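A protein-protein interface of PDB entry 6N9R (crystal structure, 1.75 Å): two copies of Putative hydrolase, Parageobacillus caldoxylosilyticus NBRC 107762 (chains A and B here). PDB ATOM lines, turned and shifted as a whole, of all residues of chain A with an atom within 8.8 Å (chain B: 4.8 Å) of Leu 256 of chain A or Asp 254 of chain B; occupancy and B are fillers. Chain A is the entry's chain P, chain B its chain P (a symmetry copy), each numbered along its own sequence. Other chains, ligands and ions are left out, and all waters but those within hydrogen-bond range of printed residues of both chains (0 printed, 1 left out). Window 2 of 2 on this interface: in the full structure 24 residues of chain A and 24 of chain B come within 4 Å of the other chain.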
ATOM      1  N   PHE A 208      25.417  28.405 -13.563  1.00  0.00           N
ATOM      2  CA  PHE A 208      24.807  27.086 -13.390  1.00  0.00           C
ATOM      3  C   PHE A 208      23.793  27.109 -12.241  1.00  0.00           C
ATOM      4  O   PHE A 208      22.816  26.362 -12.253  1.00  0.00           O
ATOM      5  CB  PHE A 208      25.873  26.020 -13.123  1.00  0.00           C
ATOM      6  CG  PHE A 208      26.686  25.606 -14.324  1.00  0.00           C
ATOM      7  CD1 PHE A 208      26.149  25.653 -15.602  1.00  0.00           C
ATOM      8  CD2 PHE A 208      27.981  25.137 -14.173  1.00  0.00           C
ATOM      9  CE1 PHE A 208      26.897  25.261 -16.701  1.00  0.00           C
ATOM     10  CE2 PHE A 208      28.728  24.744 -15.273  1.00  0.00           C
ATOM     11  CZ  PHE A 208      28.185  24.806 -16.535  1.00  0.00           C
ATOM     12  N   SER A 210      22.390  26.718  -8.245  1.00  0.00           N
ATOM     13  CA  SER A 210      22.463  25.758  -7.151  1.00  0.00           C
ATOM     14  C   SER A 210      22.444  24.326  -7.695  1.00  0.00           C
ATOM     15  O   SER A 210      21.787  24.032  -8.695  1.00  0.00           O
ATOM     16  CB  SER A 210      21.351  25.984  -6.158  1.00  0.00           C
ATOM     17  OG  SER A 210      20.083  25.955  -6.796  1.00  0.00           O
ATOM     18  N   GLY A 211      23.178  23.448  -7.008  1.00  0.00           N
ATOM     19  CA  GLY A 211      23.289  22.039  -7.349  1.00  0.00           C
ATOM     20  C   GLY A 211      24.239  21.330  -6.400  1.00  0.00           C
ATOM     21  O   GLY A 211      23.895  21.069  -5.247  1.00  0.00           O
ATOM     22  N   HIS A 212      25.445  21.039  -6.897  1.00  0.00           N
ATOM     23  CA  HIS A 212      26.527  20.491  -6.090  1.00  0.00           C
ATOM     24  C   HIS A 212      26.685  21.333  -4.819  1.00  0.00           C
ATOM     25  O   HIS A 212      26.766  20.800  -3.714  1.00  0.00           O
ATOM     26  CB  HIS A 212      27.824  20.437  -6.910  1.00  0.00           C
ATOM     27  CG  HIS A 212      29.049  20.192  -6.097  1.00  0.00           C
ATOM     28  ND1 HIS A 212      29.333  18.961  -5.540  1.00  0.00           N
ATOM     29  CD2 HIS A 212      30.072  21.007  -5.756  1.00  0.00           C
ATOM     30  CE1 HIS A 212      30.475  19.031  -4.885  1.00  0.00           C
ATOM     31  NE2 HIS A 212      30.949  20.274  -5.003  1.00  0.00           N
ATOM     32  N   ILE A 246      22.584   9.765 -15.517  1.00  0.00           N
ATOM     33  CA  ILE A 246      23.280  10.566 -14.522  1.00  0.00           C
ATOM     34  C   ILE A 246      23.399   9.755 -13.228  1.00  0.00           C
ATOM     35  O   ILE A 246      22.444   9.112 -12.797  1.00  0.00           O
ATOM     36  CB  ILE A 246      22.554  11.905 -14.285  1.00  0.00           C
ATOM     37  CG1 ILE A 246      22.483  12.745 -15.562  1.00  0.00           C
ATOM     38  CG2 ILE A 246      23.200  12.668 -13.138  1.00  0.00           C
ATOM     39  CD1 ILE A 246      21.641  13.992 -15.431  1.00  0.00           C
ATOM     40  N   PRO A 248      24.373  10.863  -9.560  1.00  0.00           N
ATOM     41  CA  PRO A 248      24.677  12.026  -8.729  1.00  0.00           C
ATOM     42  C   PRO A 248      25.605  11.711  -7.560  1.00  0.00           C
ATOM     43  O   PRO A 248      25.781  10.556  -7.182  1.00  0.00           O
ATOM     44  CB  PRO A 248      23.298  12.466  -8.218  1.00  0.00           C
ATOM     45  CG  PRO A 248      22.481  11.190  -8.212  1.00  0.00           C
ATOM     46  CD  PRO A 248      22.988  10.396  -9.399  1.00  0.00           C
ATOM     47  N   ILE A 252      24.610  16.471  -1.671  1.00  0.00           N
ATOM     48  CA  ILE A 252      24.131  17.390  -2.688  1.00  0.00           C
ATOM     49  C   ILE A 252      23.318  18.491  -2.004  1.00  0.00           C
ATOM     50  O   ILE A 252      22.476  18.200  -1.157  1.00  0.00           O
ATOM     51  CB  ILE A 252      23.284  16.613  -3.716  1.00  0.00           C
ATOM     52  CG1 ILE A 252      23.461  17.129  -5.144  1.00  0.00           C
ATOM     53  CG2 ILE A 252      21.822  16.597  -3.299  1.00  0.00           C
ATOM     54  CD1 ILE A 252      22.913  16.182  -6.187  1.00  0.00           C
ATOM     55  N   TYR A 253      23.570  19.751  -2.376  1.00  0.00           N
ATOM     56  CA  TYR A 253      22.787  20.845  -1.834  1.00  0.00           C
ATOM     57  C   TYR A 253      21.386  20.826  -2.460  1.00  0.00           C
ATOM     58  O   TYR A 253      20.386  20.723  -1.754  1.00  0.00           O
ATOM     59  CB  TYR A 253      23.442  22.208  -2.069  1.00  0.00           C
ATOM     60  CG  TYR A 253      22.530  23.349  -1.698  1.00  0.00           C
ATOM     61  CD1 TYR A 253      22.101  23.516  -0.391  1.00  0.00           C
ATOM     62  CD2 TYR A 253      22.052  24.229  -2.654  1.00  0.00           C
ATOM     63  CE1 TYR A 253      21.241  24.542  -0.038  1.00  0.00           C
ATOM     64  CE2 TYR A 253      21.192  25.263  -2.316  1.00  0.00           C
ATOM     65  CZ  TYR A 253      20.786  25.420  -1.004  1.00  0.00           C
ATOM     66  OH  TYR A 253      19.940  26.436  -0.664  1.00  0.00           O
ATOM     67  N   ASP A 254      21.344  20.925  -3.793  1.00  0.00           N
ATOM     68  CA  ASP A 254      20.105  21.039  -4.559  1.00  0.00           C
ATOM     69  C   ASP A 254      20.080  19.939  -5.627  1.00  0.00           C
ATOM     70  O   ASP A 254      20.631  20.110  -6.714  1.00  0.00           O
ATOM     71  CB  ASP A 254      19.989  22.434  -5.180  1.00  0.00           C
ATOM     72  CG  ASP A 254      18.771  22.638  -6.065  1.00  0.00           C
ATOM     73  OD1 ASP A 254      17.902  21.741  -6.086  1.00  0.00           O
ATOM     74  OD2 ASP A 254      18.703  23.695  -6.726  1.00  0.00           O
ATOM     75  N   SER A 255      19.433  18.814  -5.303  1.00  0.00           N
ATOM     76  CA  SER A 255      19.416  17.638  -6.177  1.00  0.00           C
ATOM     77  C   SER A 255      18.761  17.975  -7.522  1.00  0.00           C
ATOM     78  O   SER A 255      19.258  17.567  -8.570  1.00  0.00           O
ATOM     79  CB  SER A 255      18.738  16.466  -5.511  1.00  0.00           C
ATOM     80  OG  SER A 255      17.411  16.793  -5.128  1.00  0.00           O
ATOM     81  N   LEU A 256      17.649  18.717  -7.486  1.00  0.00           N
ATOM     82  CA  LEU A 256      16.911  19.060  -8.704  1.00  0.00           C
ATOM     83  C   LEU A 256      17.773  19.977  -9.579  1.00  0.00           C
ATOM     84  O   LEU A 256      17.873  19.777 -10.791  1.00  0.00           O
ATOM     85  CB  LEU A 256      15.585  19.735  -8.335  1.00  0.00           C
ATOM     86  CG  LEU A 256      14.569  18.842  -7.623  1.00  0.00           C
ATOM     87  CD1 LEU A 256      13.244  19.566  -7.448  1.00  0.00           C
ATOM     88  CD2 LEU A 256      14.369  17.535  -8.378  1.00  0.00           C
ATOM     89  N   GLY A 257      18.386  20.982  -8.944  1.00  0.00           N
ATOM     90  CA  GLY A 257      19.283  21.907  -9.617  1.00  0.00           C
ATOM     91  C   GLY A 257      20.472  21.184 -10.228  1.00  0.00           C
ATOM     92  O   GLY A 257      20.890  21.491 -11.346  1.00  0.00           O
ATOM     93  N   TYR A 258      21.013  20.214  -9.484  1.00  0.00           N
ATOM     94  CA  TYR A 258      22.158  19.445  -9.943  1.00  0.00           C
ATOM     95  C   TYR A 258      21.795  18.716 -11.242  1.00  0.00           C
ATOM     96  O   TYR A 258      22.530  18.786 -12.228  1.00  0.00           O
ATOM     97  CB  TYR A 258      22.626  18.446  -8.884  1.00  0.00           C
ATOM     98  CG  TYR A 258      23.630  17.454  -9.413  1.00  0.00           C
ATOM     99  CD1 TYR A 258      24.987  17.724  -9.384  1.00  0.00           C
ATOM    100  CD2 TYR A 258      23.219  16.263  -9.988  1.00  0.00           C
ATOM    101  CE1 TYR A 258      25.913  16.828  -9.891  1.00  0.00           C
ATOM    102  CE2 TYR A 258      24.132  15.355 -10.497  1.00  0.00           C
ATOM    103  CZ  TYR A 258      25.484  15.639 -10.451  1.00  0.00           C
ATOM    104  OH  TYR A 258      26.390  14.749 -10.951  1.00  0.00           O
ATOM    105  N   MET A 259      20.654  18.022 -11.227  1.00  0.00           N
ATOM    106  CA  MET A 259      20.211  17.213 -12.361  1.00  0.00           C
ATOM    107  C   MET A 259      19.963  18.119 -13.573  1.00  0.00           C
ATOM    108  O   MET A 259      20.353  17.789 -14.696  1.00  0.00           O
ATOM    109  CB  MET A 259      18.929  16.447 -12.022  1.00  0.00           C
ATOM    110  CG  MET A 259      19.113  15.424 -10.918  1.00  0.00           C
ATOM    111  SD  MET A 259      20.301  14.130 -11.360  1.00  0.00           S
ATOM    112  CE  MET A 259      19.400  13.288 -12.659  1.00  0.00           C
ATOM    113  N   ASN A 260      19.311  19.262 -13.331  1.00  0.00           N
ATOM    114  CA  ASN A 260      18.998  20.228 -14.378  1.00  0.00           C
ATOM    115  C   ASN A 260      20.298  20.736 -15.012  1.00  0.00           C
ATOM    116  O   ASN A 260      20.380  20.890 -16.229  1.00  0.00           O
ATOM    117  CB  ASN A 260      18.163  21.395 -13.847  1.00  0.00           C
ATOM    118  CG  ASN A 260      16.732  21.006 -13.539  1.00  0.00           C
ATOM    119  OD1 ASN A 260      16.214  20.037 -14.089  1.00  0.00           O
ATOM    120  ND2 ASN A 260      16.084  21.760 -12.666  1.00  0.00           N
ATOM    121  N   THR A 261      21.306  21.000 -14.173  1.00  0.00           N
ATOM    122  CA  THR A 261      22.569  21.574 -14.634  1.00  0.00           C
ATOM    123  C   THR A 261      23.292  20.579 -15.551  1.00  0.00           C
ATOM    124  O   THR A 261      23.804  20.967 -16.600  1.00  0.00           O
ATOM    125  CB  THR A 261      23.455  22.005 -13.459  1.00  0.00           C
ATOM    126  OG1 THR A 261      22.816  23.104 -12.807  1.00  0.00           O
ATOM    127  CG2 THR A 261      24.846  22.408 -13.895  1.00  0.00           C
ATOM    128  N   VAL A 262      23.329  19.304 -15.153  1.00  0.00           N
ATOM    129  CA  VAL A 262      24.012  18.277 -15.943  1.00  0.00           C
ATOM    130  C   VAL A 262      23.383  18.226 -17.339  1.00  0.00           C
ATOM    131  O   VAL A 262      24.091  18.184 -18.345  1.00  0.00           O
ATOM    132  CB  VAL A 262      23.975  16.892 -15.267  1.00  0.00           C
ATOM    133  CG1 VAL A 262      24.508  15.810 -16.196  1.00  0.00           C
ATOM    134  CG2 VAL A 262      24.728  16.879 -13.945  1.00  0.00           C
ATOM    135  N   GLU A 263      22.047  18.228 -17.387  1.00  0.00           N
ATOM    136  CA  GLU A 263      21.316  18.102 -18.647  1.00  0.00           C
ATOM    137  C   GLU A 263      21.521  19.373 -19.481  1.00  0.00           C
ATOM    138  O   GLU A 263      21.603  19.310 -20.705  1.00  0.00           O
ATOM    139  CB  GLU A 263      19.836  17.813 -18.384  1.00  0.00           C
ATOM    140  CG  GLU A 263      19.582  16.395 -17.906  1.00  0.00           C
ATOM    141  CD  GLU A 263      20.237  15.316 -18.752  1.00  0.00           C
ATOM    142  OE1 GLU A 263      20.492  15.575 -19.945  1.00  0.00           O
ATOM    143  OE2 GLU A 263      20.494  14.219 -18.215  1.00  0.00           O
ATOM    144  N   SER B 210       7.290  17.707  -3.032  1.00  0.00           N
ATOM    145  CA  SER B 210       8.480  16.959  -3.420  1.00  0.00           C
ATOM    146  C   SER B 210       9.526  17.003  -2.301  1.00  0.00           C
ATOM    147  O   SER B 210       9.662  18.002  -1.593  1.00  0.00           O
ATOM    148  CB  SER B 210       9.043  17.475  -4.720  1.00  0.00           C
ATOM    149  OG  SER B 210       9.302  18.870  -4.646  1.00  0.00           O
ATOM    150  N   GLY B 211      10.260  15.896  -2.167  1.00  0.00           N
ATOM    151  CA  GLY B 211      11.311  15.734  -1.175  1.00  0.00           C
ATOM    152  C   GLY B 211      11.915  14.343  -1.255  1.00  0.00           C
ATOM    153  O   GLY B 211      12.675  14.041  -2.175  1.00  0.00           O
ATOM    154  N   ILE B 252      17.648  10.950  -2.569  1.00  0.00           N
ATOM    155  CA  ILE B 252      16.668  12.002  -2.368  1.00  0.00           C
ATOM    156  C   ILE B 252      16.260  12.554  -3.735  1.00  0.00           C
ATOM    157  O   ILE B 252      17.117  12.823  -4.573  1.00  0.00           O
ATOM    158  CB  ILE B 252      17.278  13.099  -1.472  1.00  0.00           C
ATOM    159  CG1 ILE B 252      16.261  13.720  -0.515  1.00  0.00           C
ATOM    160  CG2 ILE B 252      17.972  14.154  -2.319  1.00  0.00           C
ATOM    161  CD1 ILE B 252      16.904  14.539   0.582  1.00  0.00           C
ATOM    162  N   TYR B 253      14.951  12.722  -3.955  1.00  0.00           N
ATOM    163  CA  TYR B 253      14.486  13.315  -5.195  1.00  0.00           C
ATOM    164  C   TYR B 253      14.789  14.819  -5.184  1.00  0.00           C
ATOM    165  O   TYR B 253      15.492  15.323  -6.056  1.00  0.00           O
ATOM    166  CB  TYR B 253      12.991  13.087  -5.430  1.00  0.00           C
ATOM    167  CG  TYR B 253      12.472  13.880  -6.601  1.00  0.00           C
ATOM    168  CD1 TYR B 253      12.950  13.648  -7.881  1.00  0.00           C
ATOM    169  CD2 TYR B 253      11.548  14.897  -6.430  1.00  0.00           C
ATOM    170  CE1 TYR B 253      12.505  14.386  -8.964  1.00  0.00           C
ATOM    171  CE2 TYR B 253      11.090  15.643  -7.505  1.00  0.00           C
ATOM    172  CZ  TYR B 253      11.570  15.387  -8.777  1.00  0.00           C
ATOM    173  OH  TYR B 253      11.124  16.118  -9.840  1.00  0.00           O
ATOM    174  N   ASP B 254      14.244  15.513  -4.179  1.00  0.00           N
ATOM    175  CA  ASP B 254      14.323  16.967  -4.062  1.00  0.00           C
ATOM    176  C   ASP B 254      14.898  17.324  -2.686  1.00  0.00           C
ATOM    177  O   ASP B 254      14.163  17.400  -1.702  1.00  0.00           O
ATOM    178  CB  ASP B 254      12.942  17.595  -4.278  1.00  0.00           C
ATOM    179  CG  ASP B 254      12.894  19.103  -4.102  1.00  0.00           C
ATOM    180  OD1 ASP B 254      13.974  19.715  -3.962  1.00  0.00           O
ATOM    181  OD2 ASP B 254      11.773  19.654  -4.106  1.00  0.00           O
ATOM    182  N   SER B 255      16.217  17.540  -2.634  1.00  0.00           N
ATOM    183  CA  SER B 255      16.925  17.782  -1.374  1.00  0.00           C
ATOM    184  C   SER B 255      16.393  19.050  -0.692  1.00  0.00           C
ATOM    185  O   SER B 255      16.190  19.060   0.520  1.00  0.00           O
ATOM    186  CB  SER B 255      18.417  17.854  -1.584  1.00  0.00           C
ATOM    187  OG  SER B 255      18.754  18.865  -2.521  1.00  0.00           O
ATOM    188  N   LEU B 256      16.171  20.112  -1.475  1.00  0.00           N
ATOM    189  CA  LEU B 256      15.709  21.390  -0.928  1.00  0.00           C
ATOM    190  C   LEU B 256      14.296  21.219  -0.362  1.00  0.00           C
ATOM    191  O   LEU B 256      13.999  21.684   0.740  1.00  0.00           O
ATOM    192  CB  LEU B 256      15.742  22.464  -2.021  1.00  0.00           C
ATOM    193  CG  LEU B 256      17.133  22.849  -2.522  1.00  0.00           C
ATOM    194  CD1 LEU B 256      17.054  24.025  -3.484  1.00  0.00           C
ATOM    195  CD2 LEU B 256      18.062  23.171  -1.361  1.00  0.00           C
ATOM    196  N   GLY B 257      13.434  20.550  -1.136  1.00  0.00           N
ATOM    197  CA  GLY B 257      12.072  20.254  -0.723  1.00  0.00           C
ATOM    198  C   GLY B 257      12.045  19.407   0.538  1.00  0.00           C
ATOM    199  O   GLY B 257      11.230  19.635   1.434  1.00  0.00           O
ATOM    200  N   TYR B 258      12.948  18.424   0.602  1.00  0.00           N
ATOM    201  CA  TYR B 258      13.031  17.532   1.747  1.00  0.00           C
ATOM    202  C   TYR B 258      13.327  18.352   3.010  1.00  0.00           C
ATOM    203  O   TYR B 258      12.649  18.204   4.027  1.00  0.00           O
ATOM    204  CB  TYR B 258      14.098  16.455   1.548  1.00  0.00           C
ATOM    205  CG  TYR B 258      14.399  15.684   2.808  1.00  0.00           C
ATOM    206  CD1 TYR B 258      13.684  14.545   3.137  1.00  0.00           C
ATOM    207  CD2 TYR B 258      15.369  16.119   3.695  1.00  0.00           C
ATOM    208  CE1 TYR B 258      13.938  13.846   4.305  1.00  0.00           C
ATOM    209  CE2 TYR B 258      15.637  15.430   4.865  1.00  0.00           C
ATOM    210  CZ  TYR B 258      14.919  14.291   5.173  1.00  0.00           C
ATOM    211  OH  TYR B 258      15.177  13.605   6.325  1.00  0.00           O
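OG of Ser 255 of chain B touches CG2 of Ile 252 of chain A, 3.9 Å away. O of Tyr 253 of chain A touches CD2 of Leu 256 of chain B, 3.4 Å away. Asp 254 of chain A touches Ser 255 of chain B (CA to OG, 3.3 Å). Leu 256 of chain B touches Asp 254 of chain A (CD1 to CG, 3.4 Å). OG of Ser 255 of chain A touches CG2 of Ile 252 of chain B, at 3.9 Å. Ser 255 of chain A touches Asp 254 of chain B (OG to CA, 3.3 Å). Leu 256 of chain A touches Tyr 253 of chain B. Leu 256 of chain A touches Asp 254 of chain B.
OD2 of Asp 254 of chain A is in hydrogen-bond range of OG of Ser 210 of chain A (2.6 Å). N of Tyr 253 of chain A sits at hydrogen-bond distance from O of Gly 211 of chain A (3.2 Å). The side-chain amide nitrogen (ND2) of Asn 260 of chain A lies close to the backbone carbonyl oxygen (O) of Leu 256 of chain A. The backbone NH of Tyr 253 of chain B is in hydrogen-bond range of the backbone carbonyl oxygen of Gly 211 of chain B. O of Gly 211 of chain B lies within hydrogen-bond range of N of Asp 254 of chain B (2.9 Å). The side-chain carboxylate (OD1) of Asp 254 of chain B lies close to the backbone NH (N) of Leu 256 of chain B (3.3 Å).
Hydrophobic or aromatic side chains of chain B within 4 Å of the printed part of chain A: Ile 252, Tyr 253 and Leu 256. Along chain B the printed residues that touch a printed residue of chain A span positions 252 to 256. Of the 18 printed residues of chain A, 5 touch a printed residue of chain B. Hydrophobic or aromatic side chains of chain A within 4 Å of the printed part of chain B: Ile 252, Tyr 253 and Leu 256. Among the printed residues, no Asp or Glu carboxylate lies within 4 Å of a Lys or Arg side-chain nitrogen of the other chain.
The side-chain hydroxyl of Ser 255 of chain B is in hydrogen-bond range of the backbone carbonyl oxygen of Tyr 253 of chain A, 2.6 Å away. The side-chain hydroxyl (OG) of Ser 255 of chain A lies within hydrogen-bond range of the backbone carbonyl oxygen (O) of Tyr 253 of chain B. N of Ser 255 of chain A is in hydrogen-bond range of OG of Ser 255 of chain B.
Ile 246 of chain A touches none of the printed residues of chain B. Of the printed residues of chain B, Tyr 253 of chain A touches Ser 255 (2.6 Å) and Leu 256 (3.4 Å). Printed residues of chain B within 4 Å of Asp 254 of chain A: Ser 255 and Leu 256. Of chain B, only Tyr 253 and Asp 254 come within 4 Å of Leu 256 of chain A. Gly 257 of chain A touches none of the printed residues of chain B. No residue of chain A comes within 4 Å of Gly 211 of chain B. Printed residues of chain A within 4 Å of Ile 252 of chain B: Ser 255 (3.9 Å). Printed residues of chain A within 4 Å of Tyr 253 of chain B: Ser 255 (2.6 Å) and Leu 256 (3.4 Å). The nearest printed residue of chain B that does not touch Leu 256 of chain A is Ser 210 of chain B (4.9 Å). The nearest residue of chain A that does not touch Asp 254 of chain B is Asp 254 of chain A (4.9 Å).
Ile 252 of chain A touches Ser 255 of chain B, and with the chains exchanged Ser 255 of chain A touches Ile 252 of chain B. Tyr 253 of chain A touches Ser 255 of chain B, and with the chains exchanged Ser 255 of chain A touches Tyr 253 of chain B. Asp 254 of chain A touches Ser 255 of chain B, and with the chains exchanged Ser 255 of chain A touches Asp 254 of chain B. Asp 254 of chain A touches Leu 256 of chain B, and with the chains exchanged Leu 256 of chain A touches Asp 254 of chain B. Of the 11 pairs that touch across the chains among the printed residues, 11 have their exchanged pair printed and touching as well.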
